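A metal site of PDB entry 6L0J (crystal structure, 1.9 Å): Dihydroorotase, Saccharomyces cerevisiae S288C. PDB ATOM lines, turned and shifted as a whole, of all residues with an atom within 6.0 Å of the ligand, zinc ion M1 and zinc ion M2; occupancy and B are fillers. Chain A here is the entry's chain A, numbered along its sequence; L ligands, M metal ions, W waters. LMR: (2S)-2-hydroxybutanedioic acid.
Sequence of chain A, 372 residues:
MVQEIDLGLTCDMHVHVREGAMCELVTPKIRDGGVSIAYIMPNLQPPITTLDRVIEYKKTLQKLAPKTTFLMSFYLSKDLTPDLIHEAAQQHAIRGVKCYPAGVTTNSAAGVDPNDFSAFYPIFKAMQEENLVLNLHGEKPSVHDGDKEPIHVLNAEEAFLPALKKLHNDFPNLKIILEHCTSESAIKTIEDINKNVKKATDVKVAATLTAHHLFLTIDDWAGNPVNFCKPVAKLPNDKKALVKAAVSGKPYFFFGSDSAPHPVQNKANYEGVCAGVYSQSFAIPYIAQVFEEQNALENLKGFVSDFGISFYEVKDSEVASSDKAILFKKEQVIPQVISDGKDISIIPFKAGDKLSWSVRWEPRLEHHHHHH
Within 4 Å of zinc ion M1: His 14, His 16, KCX 98 and Asp 258.
Zinc ion M1 is bound by a ring nitrogen (NE2) of His 14 (2.0 Å), the side-chain carboxylate of Asp 258 (2.1 Å), OQ2 of KCX 98 (2.1 Å), an oxygen (O1A) of the ligand (2.1 Å) and a ring nitrogen (NE2) of His 16 (2.1 Å).
Zinc ion M1 has five donor atoms within binding distance.
Merely in contact with the ligand: Lys 230 and Ala 260.
Hydrophobic or aromatic side chains that line the ligand: His 16, His 137, Ala 260 and His 262.
14 residues have an atom within 4 Å of the ligand: His 14, His 16, Arg 18, Asn 43, KCX 98, Thr 105, Thr 106, His 137, His 180, Lys 230, Asp 258, Ala 260, His 262 and Ala 275.
The nearest printed residue that does not touch the ligand is Gly 276 (4.2 Å).
NZ of KCX 98 is in hydrogen-bond range of the side-chain sulfur of Met 41 (3.5 Å).
NZ of KCX 98 is in hydrogen-bond range of OH of Tyr 100 (3.0 Å).
The side-chain amide oxygen (OD1) of Asn 43 sits at hydrogen-bond distance from a ring nitrogen (ND1) of His 16 (2.8 Å).
The backbone NH of His 16 lies within hydrogen-bond range of the backbone carbonyl oxygen of Ser 259, at 3.2 Å.
O of Pro 261 lies within hydrogen-bond range of NE of Arg 18, at 2.8 Å.
The backbone carbonyl oxygen (O) of Thr 106 is in hydrogen-bond range of the side-chain amide nitrogen (ND2) of Asn 43, 3.2 Å away.
The side-chain hydroxyl (OG1) of Thr 106 lies within hydrogen-bond range of the backbone carbonyl oxygen (O) of Ala 275, 3.2 Å away.
The backbone carbonyl oxygen of Ala 275 sits at hydrogen-bond distance from a ring nitrogen (NE2) of His 262 (2.7 Å).
The side-chain hydroxyl (OG1) of Thr 105 is in hydrogen-bond range of an oxygen (O1B) of the ligand (2.5 Å).
The guanidinium group of Arg 18 lies within salt-bridge range of an oxygen (O4B) of the ligand.
An oxygen (O4B) of the ligand lies within hydrogen-bond range of the side-chain amide nitrogen of Asn 43 (2.5 Å).
The side-chain hydroxyl of Thr 106 sits at hydrogen-bond distance from an oxygen (O4A) of the ligand (2.9 Å).
An oxygen (O2) of the ligand is in hydrogen-bond range of the backbone carbonyl oxygen of Ala 275 (3.1 Å).
An oxygen (O4A) of the ligand sits at hydrogen-bond distance from a ring nitrogen (NE2) of His 262 (3.3 Å).
OQ1 of KCX 98 binds zinc ion M2 (2.0 Å).
A ring nitrogen (ND1) of His 137 binds zinc ion M2 (2.0 Å).
Zinc ion M2 is bound by NE2 of His 180 (2.1 Å).
O1A of the ligand is bound to zinc ion M2 (2.5 Å).
Zinc ion M2 has four donor atoms within binding distance.
Slightly farther from zinc ion M2 lies O1B of the ligand (2.8 Å).
Water W1 lies within hydrogen-bond range of O of Lys 230, O2 of the ligand and OD2 of Asp 258.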
ATOM      1  N   HIS A  14       3.152  -5.631  15.989  1.00  0.00           N
ATOM      2  CA  HIS A  14       1.899  -5.994  16.675  1.00  0.00           C
ATOM      3  C   HIS A  14       2.203  -6.192  18.162  1.00  0.00           C
ATOM      4  O   HIS A  14       2.509  -7.306  18.593  1.00  0.00           O
ATOM      5  CB  HIS A  14       1.266  -7.232  16.051  1.00  0.00           C
ATOM      6  CG  HIS A  14      -0.135  -7.509  16.511  1.00  0.00           C
ATOM      7  ND1 HIS A  14      -1.141  -7.924  15.662  1.00  0.00           N
ATOM      8  CD2 HIS A  14      -0.705  -7.408  17.742  1.00  0.00           C
ATOM      9  CE1 HIS A  14      -2.265  -8.078  16.353  1.00  0.00           C
ATOM     10  NE2 HIS A  14      -2.021  -7.773  17.617  1.00  0.00           N
ATOM     11  N   HIS A  16       1.112  -5.338  22.295  1.00  0.00           N
ATOM     12  CA  HIS A  16       0.258  -4.871  23.387  1.00  0.00           C
ATOM     13  C   HIS A  16       1.102  -4.576  24.613  1.00  0.00           C
ATOM     14  O   HIS A  16       1.851  -5.447  25.081  1.00  0.00           O
ATOM     15  CB  HIS A  16      -0.820  -5.907  23.740  1.00  0.00           C
ATOM     16  CG  HIS A  16      -1.725  -6.243  22.605  1.00  0.00           C
ATOM     17  ND1 HIS A  16      -2.933  -5.621  22.405  1.00  0.00           N
ATOM     18  CD2 HIS A  16      -1.592  -7.150  21.602  1.00  0.00           C
ATOM     19  CE1 HIS A  16      -3.517  -6.130  21.329  1.00  0.00           C
ATOM     20  NE2 HIS A  16      -2.726  -7.060  20.832  1.00  0.00           N
ATOM     21  N   ARG A  18      -0.529  -2.650  27.319  1.00  0.00           N
ATOM     22  CA  ARG A  18      -1.523  -2.415  28.379  1.00  0.00           C
ATOM     23  C   ARG A  18      -1.298  -1.010  28.978  1.00  0.00           C
ATOM     24  O   ARG A  18      -0.861  -0.087  28.285  1.00  0.00           O
ATOM     25  CB  ARG A  18      -1.468  -3.532  29.424  1.00  0.00           C
ATOM     26  CG  ARG A  18      -1.397  -4.965  28.861  1.00  0.00           C
ATOM     27  CD  ARG A  18      -2.662  -5.345  28.044  1.00  0.00           C
ATOM     28  NE  ARG A  18      -2.648  -6.777  27.762  1.00  0.00           N
ATOM     29  CZ  ARG A  18      -3.245  -7.355  26.725  1.00  0.00           C
ATOM     30  NH1 ARG A  18      -3.929  -6.628  25.838  1.00  0.00           N
ATOM     31  NH2 ARG A  18      -3.170  -8.675  26.598  1.00  0.00           N
ATOM     32  N   MET A  41      -0.903  -1.573  19.708  1.00  0.00           N
ATOM     33  CA  MET A  41      -2.320  -1.833  19.488  1.00  0.00           C
ATOM     34  C   MET A  41      -3.180  -1.057  20.478  1.00  0.00           C
ATOM     35  O   MET A  41      -2.732  -0.703  21.569  1.00  0.00           O
ATOM     36  CB  MET A  41      -2.600  -3.326  19.598  1.00  0.00           C
ATOM     37  CG  MET A  41      -2.020  -4.103  18.409  1.00  0.00           C
ATOM     38  SD  MET A  41      -2.704  -3.458  16.837  1.00  0.00           S
ATOM     39  CE  MET A  41      -1.627  -4.234  15.611  1.00  0.00           C
ATOM     40  N   ASN A  43      -6.421  -1.685  21.930  1.00  0.00           N
ATOM     41  CA  ASN A  43      -7.511  -2.331  22.669  1.00  0.00           C
ATOM     42  C   ASN A  43      -7.341  -2.204  24.192  1.00  0.00           C
ATOM     43  O   ASN A  43      -7.335  -3.196  24.939  1.00  0.00           O
ATOM     44  CB  ASN A  43      -7.640  -3.786  22.242  1.00  0.00           C
ATOM     45  CG  ASN A  43      -6.413  -4.617  22.603  1.00  0.00           C
ATOM     46  OD1 ASN A  43      -5.292  -4.090  22.652  1.00  0.00           O
ATOM     47  ND2 ASN A  43      -6.606  -5.906  22.885  1.00  0.00           N
ATOM     48  N   KCX A  98      -6.861  -0.115  13.961  1.00  0.00           N
ATOM     49  CA  KCX A  98      -6.988  -1.561  14.115  1.00  0.00           C
ATOM     50  CB  KCX A  98      -6.155  -2.029  15.324  1.00  0.00           C
ATOM     51  CG  KCX A  98      -6.392  -3.484  15.770  1.00  0.00           C
ATOM     52  CD  KCX A  98      -5.792  -4.452  14.756  1.00  0.00           C
ATOM     53  CE  KCX A  98      -5.876  -5.835  15.295  1.00  0.00           C
ATOM     54  NZ  KCX A  98      -5.207  -5.846  16.622  1.00  0.00           N
ATOM     55  C   KCX A  98      -8.443  -1.962  14.292  1.00  0.00           C
ATOM     56  O   KCX A  98      -9.161  -1.411  15.137  1.00  0.00           O
ATOM     57  CX  KCX A  98      -5.062  -6.991  17.286  1.00  0.00           C
ATOM     58  OQ1 KCX A  98      -5.459  -8.079  16.782  1.00  0.00           O
ATOM     59  OQ2 KCX A  98      -4.509  -6.965  18.400  1.00  0.00           O
ATOM     60  N   TYR A 100     -11.161  -4.738  15.475  1.00  0.00           N
ATOM     61  CA  TYR A 100     -11.522  -5.916  16.255  1.00  0.00           C
ATOM     62  C   TYR A 100     -12.974  -6.240  15.975  1.00  0.00           C
ATOM     63  O   TYR A 100     -13.862  -5.455  16.357  1.00  0.00           O
ATOM     64  CB  TYR A 100     -11.340  -5.664  17.759  1.00  0.00           C
ATOM     65  CG  TYR A 100      -9.901  -5.392  18.161  1.00  0.00           C
ATOM     66  CD1 TYR A 100      -9.059  -6.445  18.508  1.00  0.00           C
ATOM     67  CD2 TYR A 100      -9.407  -4.117  18.198  1.00  0.00           C
ATOM     68  CE1 TYR A 100      -7.743  -6.211  18.871  1.00  0.00           C
ATOM     69  CE2 TYR A 100      -8.082  -3.859  18.574  1.00  0.00           C
ATOM     70  CZ  TYR A 100      -7.260  -4.917  18.916  1.00  0.00           C
ATOM     71  OH  TYR A 100      -5.951  -4.694  19.258  1.00  0.00           O
ATOM     72  N   VAL A 104     -14.579 -11.240  19.578  1.00  0.00           N
ATOM     73  CA  VAL A 104     -13.678 -12.337  19.234  1.00  0.00           C
ATOM     74  C   VAL A 104     -12.401 -12.362  20.070  1.00  0.00           C
ATOM     75  O   VAL A 104     -11.686 -13.381  20.049  1.00  0.00           O
ATOM     76  CB  VAL A 104     -13.276 -12.365  17.737  1.00  0.00           C
ATOM     77  CG1 VAL A 104     -14.523 -12.396  16.837  1.00  0.00           C
ATOM     78  CG2 VAL A 104     -12.390 -11.184  17.364  1.00  0.00           C
ATOM     79  N   THR A 105     -12.068 -11.293  20.785  1.00  0.00           N
ATOM     80  CA  THR A 105     -10.814 -11.331  21.551  1.00  0.00           C
ATOM     81  C   THR A 105     -10.817 -10.292  22.668  1.00  0.00           C
ATOM     82  O   THR A 105     -11.838  -9.650  22.943  1.00  0.00           O
ATOM     83  CB  THR A 105      -9.607 -11.137  20.611  1.00  0.00           C
ATOM     84  OG1 THR A 105      -8.399 -11.423  21.347  1.00  0.00           O
ATOM     85  CG2 THR A 105      -9.564  -9.713  20.046  1.00  0.00           C
ATOM     86  N   THR A 106      -9.669 -10.144  23.323  1.00  0.00           N
ATOM     87  CA  THR A 106      -9.521  -9.261  24.476  1.00  0.00           C
ATOM     88  C   THR A 106      -9.979  -7.835  24.167  1.00  0.00           C
ATOM     89  O   THR A 106      -9.509  -7.223  23.212  1.00  0.00           O
ATOM     90  CB  THR A 106      -8.061  -9.220  24.920  1.00  0.00           C
ATOM     91  OG1 THR A 106      -7.611 -10.559  25.220  1.00  0.00           O
ATOM     92  CG2 THR A 106      -7.886  -8.278  26.133  1.00  0.00           C
ATOM     93  N   ASN A 107     -10.884  -7.312  24.991  1.00  0.00           N
ATOM     94  CA  ASN A 107     -11.316  -5.916  24.887  1.00  0.00           C
ATOM     95  C   ASN A 107     -11.902  -5.614  23.516  1.00  0.00           C
ATOM     96  O   ASN A 107     -11.651  -4.552  22.940  1.00  0.00           O
ATOM     97  CB  ASN A 107     -10.164  -4.953  25.204  1.00  0.00           C
ATOM     98  CG  ASN A 107      -9.721  -5.002  26.656  1.00  0.00           C
ATOM     99  OD1 ASN A 107     -10.455  -5.480  27.512  1.00  0.00           O
ATOM    100  ND2 ASN A 107      -8.515  -4.517  26.948  1.00  0.00           N
ATOM    101  N   HIS A 137      -7.849  -7.744  12.841  1.00  0.00           N
ATOM    102  CA  HIS A 137      -7.975  -9.039  13.536  1.00  0.00           C
ATOM    103  C   HIS A 137      -9.037  -9.802  12.752  1.00  0.00           C
ATOM    104  O   HIS A 137     -10.240  -9.663  12.972  1.00  0.00           O
ATOM    105  CB  HIS A 137      -8.356  -8.879  15.014  1.00  0.00           C
ATOM    106  CG  HIS A 137      -8.467 -10.190  15.758  1.00  0.00           C
ATOM    107  ND1 HIS A 137      -7.632 -10.536  16.807  1.00  0.00           N
ATOM    108  CD2 HIS A 137      -9.291 -11.255  15.569  1.00  0.00           C
ATOM    109  CE1 HIS A 137      -7.939 -11.758  17.230  1.00  0.00           C
ATOM    110  NE2 HIS A 137      -8.946 -12.209  16.496  1.00  0.00           N
ATOM    111  N   GLU A 179      -3.567  -9.332  10.438  1.00  0.00           N
ATOM    112  CA  GLU A 179      -2.691  -9.544  11.572  1.00  0.00           C
ATOM    113  C   GLU A 179      -2.646 -11.025  11.920  1.00  0.00           C
ATOM    114  O   GLU A 179      -3.575 -11.770  11.657  1.00  0.00           O
ATOM    115  CB  GLU A 179      -3.197  -8.763  12.805  1.00  0.00           C
ATOM    116  CG  GLU A 179      -3.114  -7.244  12.680  1.00  0.00           C
ATOM    117  CD  GLU A 179      -1.676  -6.728  12.465  1.00  0.00           C
ATOM    118  OE1 GLU A 179      -0.716  -7.420  12.862  1.00  0.00           O
ATOM    119  OE2 GLU A 179      -1.510  -5.645  11.887  1.00  0.00           O
ATOM    120  N   HIS A 180      -1.551 -11.425  12.575  1.00  0.00           N
ATOM    121  CA  HIS A 180      -1.341 -12.762  13.126  1.00  0.00           C
ATOM    122  C   HIS A 180      -2.083 -13.883  12.394  1.00  0.00           C
ATOM    123  O   HIS A 180      -3.050 -14.455  12.916  1.00  0.00           O
ATOM    124  CB  HIS A 180      -1.674 -12.782  14.641  1.00  0.00           C
ATOM    125  CG  HIS A 180      -2.972 -12.118  15.036  1.00  0.00           C
ATOM    126  ND1 HIS A 180      -4.155 -12.237  14.340  1.00  0.00           N
ATOM    127  CD2 HIS A 180      -3.272 -11.362  16.134  1.00  0.00           C
ATOM    128  CE1 HIS A 180      -5.116 -11.579  14.965  1.00  0.00           C
ATOM    129  NE2 HIS A 180      -4.603 -11.031  16.059  1.00  0.00           N
ATOM    130  N   CYS A 229      -4.527 -18.232  22.941  1.00  0.00           N
ATOM    131  CA  CYS A 229      -4.555 -16.904  22.355  1.00  0.00           C
ATOM    132  C   CYS A 229      -5.644 -16.906  21.294  1.00  0.00           C
ATOM    133  O   CYS A 229      -6.242 -17.950  20.981  1.00  0.00           O
ATOM    134  CB  CYS A 229      -3.182 -16.508  21.780  1.00  0.00           C
ATOM    135  SG  CYS A 229      -2.590 -17.559  20.371  1.00  0.00           S
ATOM    136  N   LYS A 230      -5.961 -15.714  20.776  1.00  0.00           N
ATOM    137  CA  LYS A 230      -6.777 -15.547  19.583  1.00  0.00           C
ATOM    138  C   LYS A 230      -5.942 -14.892  18.493  1.00  0.00           C
ATOM    139  O   LYS A 230      -5.155 -13.978  18.782  1.00  0.00           O
ATOM    140  CB  LYS A 230      -8.034 -14.687  19.855  1.00  0.00           C
ATOM    141  CG  LYS A 230      -9.033 -15.287  20.862  1.00  0.00           C
ATOM    142  CD  LYS A 230      -9.465 -16.737  20.543  1.00  0.00           C
ATOM    143  CE  LYS A 230     -10.310 -16.831  19.296  1.00  0.00           C
ATOM    144  NZ  LYS A 230     -11.647 -16.189  19.495  1.00  0.00           N
ATOM    145  N   PRO A 231      -6.051 -15.353  17.217  1.00  0.00           N
ATOM    146  CA  PRO A 231      -6.797 -16.533  16.813  1.00  0.00           C
ATOM    147  C   PRO A 231      -6.079 -17.745  17.408  1.00  0.00           C
ATOM    148  O   PRO A 231      -4.881 -17.626  17.635  1.00  0.00           O
ATOM    149  CB  PRO A 231      -6.718 -16.532  15.254  1.00  0.00           C
ATOM    150  CG  PRO A 231      -6.094 -15.183  14.895  1.00  0.00           C
ATOM    151  CD  PRO A 231      -5.271 -14.783  16.106  1.00  0.00           C
ATOM    152  N   ASP A 258       2.207 -10.045  18.439  1.00  0.00           N
ATOM    153  CA  ASP A 258       1.012 -10.104  19.281  1.00  0.00           C
ATOM    154  C   ASP A 258       1.391 -10.522  20.699  1.00  0.00           C
ATOM    155  O   ASP A 258       0.654 -11.284  21.338  1.00  0.00           O
ATOM    156  CB  ASP A 258      -0.062 -11.055  18.738  1.00  0.00           C
ATOM    157  CG  ASP A 258      -1.451 -10.807  19.365  1.00  0.00           C
ATOM    158  OD1 ASP A 258      -1.695  -9.659  19.816  1.00  0.00           O
ATOM    159  OD2 ASP A 258      -2.290 -11.735  19.443  1.00  0.00           O
ATOM    160  N   SER A 259       2.502 -10.002  21.225  1.00  0.00           N
ATOM    161  CA  SER A 259       2.763 -10.218  22.638  1.00  0.00           C
ATOM    162  C   SER A 259       1.641  -9.565  23.432  1.00  0.00           C
ATOM    163  O   SER A 259       1.375  -8.380  23.279  1.00  0.00           O
ATOM    164  CB  SER A 259       4.120  -9.654  23.045  1.00  0.00           C
ATOM    165  OG  SER A 259       4.320  -9.852  24.441  1.00  0.00           O
ATOM    166  N   ALA A 260       0.945 -10.370  24.225  1.00  0.00           N
ATOM    167  CA  ALA A 260      -0.342  -9.989  24.826  1.00  0.00           C
ATOM    168  C   ALA A 260      -0.299 -10.338  26.310  1.00  0.00           C
ATOM    169  O   ALA A 260      -0.787 -11.390  26.726  1.00  0.00           O
ATOM    170  CB  ALA A 260      -1.500 -10.698  24.147  1.00  0.00           C
ATOM    171  N   PRO A 261       0.279  -9.467  27.126  1.00  0.00           N
ATOM    172  CA  PRO A 261       0.511  -9.845  28.525  1.00  0.00           C
ATOM    173  C   PRO A 261      -0.744  -9.808  29.383  1.00  0.00           C
ATOM    174  O   PRO A 261      -1.574  -8.903  29.296  1.00  0.00           O
ATOM    175  CB  PRO A 261       1.547  -8.808  29.005  1.00  0.00           C
ATOM    176  CG  PRO A 261       1.452  -7.685  28.076  1.00  0.00           C
ATOM    177  CD  PRO A 261       0.995  -8.244  26.751  1.00  0.00           C
ATOM    178  N   HIS A 262      -0.882 -10.844  30.214  1.00  0.00           N
ATOM    179  CA  HIS A 262      -1.912 -10.951  31.215  1.00  0.00           C
ATOM    180  C   HIS A 262      -1.269 -11.424  32.509  1.00  0.00           C
ATOM    181  O   HIS A 262      -0.350 -12.245  32.467  1.00  0.00           O
ATOM    182  CB  HIS A 262      -3.002 -11.965  30.817  1.00  0.00           C
ATOM    183  CG  HIS A 262      -3.770 -11.581  29.599  1.00  0.00           C
ATOM    184  ND1 HIS A 262      -4.758 -10.620  29.614  1.00  0.00           N
ATOM    185  CD2 HIS A 262      -3.707 -12.033  28.325  1.00  0.00           C
ATOM    186  CE1 HIS A 262      -5.267 -10.490  28.399  1.00  0.00           C
ATOM    187  NE2 HIS A 262      -4.634 -11.331  27.598  1.00  0.00           N
ATOM    188  N   ALA A 275      -7.328 -14.494  26.635  1.00  0.00           N
ATOM    189  CA  ALA A 275      -6.588 -14.907  25.458  1.00  0.00           C
ATOM    190  C   ALA A 275      -5.326 -14.069  25.331  1.00  0.00           C
ATOM    191  O   ALA A 275      -5.391 -12.842  25.432  1.00  0.00           O
ATOM    192  CB  ALA A 275      -7.442 -14.747  24.211  1.00  0.00           C
ATOM    193  N   GLY A 276      -4.189 -14.704  25.075  1.00  0.00           N
ATOM    194  CA  GLY A 276      -2.956 -13.941  24.889  1.00  0.00           C
ATOM    195  C   GLY A 276      -1.694 -14.642  25.378  1.00  0.00           C
ATOM    196  O   GLY A 276      -1.669 -15.224  26.465  1.00  0.00           O
HETATM  197  C1  LMR L   1      -5.467 -10.244  20.369  1.00  0.00           C
HETATM  198  O1A LMR L   1      -4.628  -9.759  19.554  1.00  0.00           O
HETATM  199  O1B LMR L   1      -6.425 -10.886  19.878  1.00  0.00           O
HETATM  200  C2  LMR L   1      -5.454 -10.076  21.909  1.00  0.00           C
HETATM  201  O2  LMR L   1      -5.366 -11.260  22.720  1.00  0.00           O
HETATM  202  C3  LMR L   1      -4.295  -9.271  22.365  1.00  0.00           C
HETATM  203  C4  LMR L   1      -4.791  -8.872  23.752  1.00  0.00           C
HETATM  204  O4A LMR L   1      -4.923  -9.713  24.710  1.00  0.00           O
HETATM  205  O4B LMR L   1      -5.083  -7.683  23.849  1.00  0.00           O
HETATM  206 ZN    ZN M   1      -3.139  -8.325  19.200  1.00  0.00          ZN
HETATM  207 ZN    ZN M   2      -5.768  -9.918  17.387  1.00  0.00          ZN
HETATM  208  O   HOH W   1      -4.105 -13.292  21.194  1.00  0.00           O
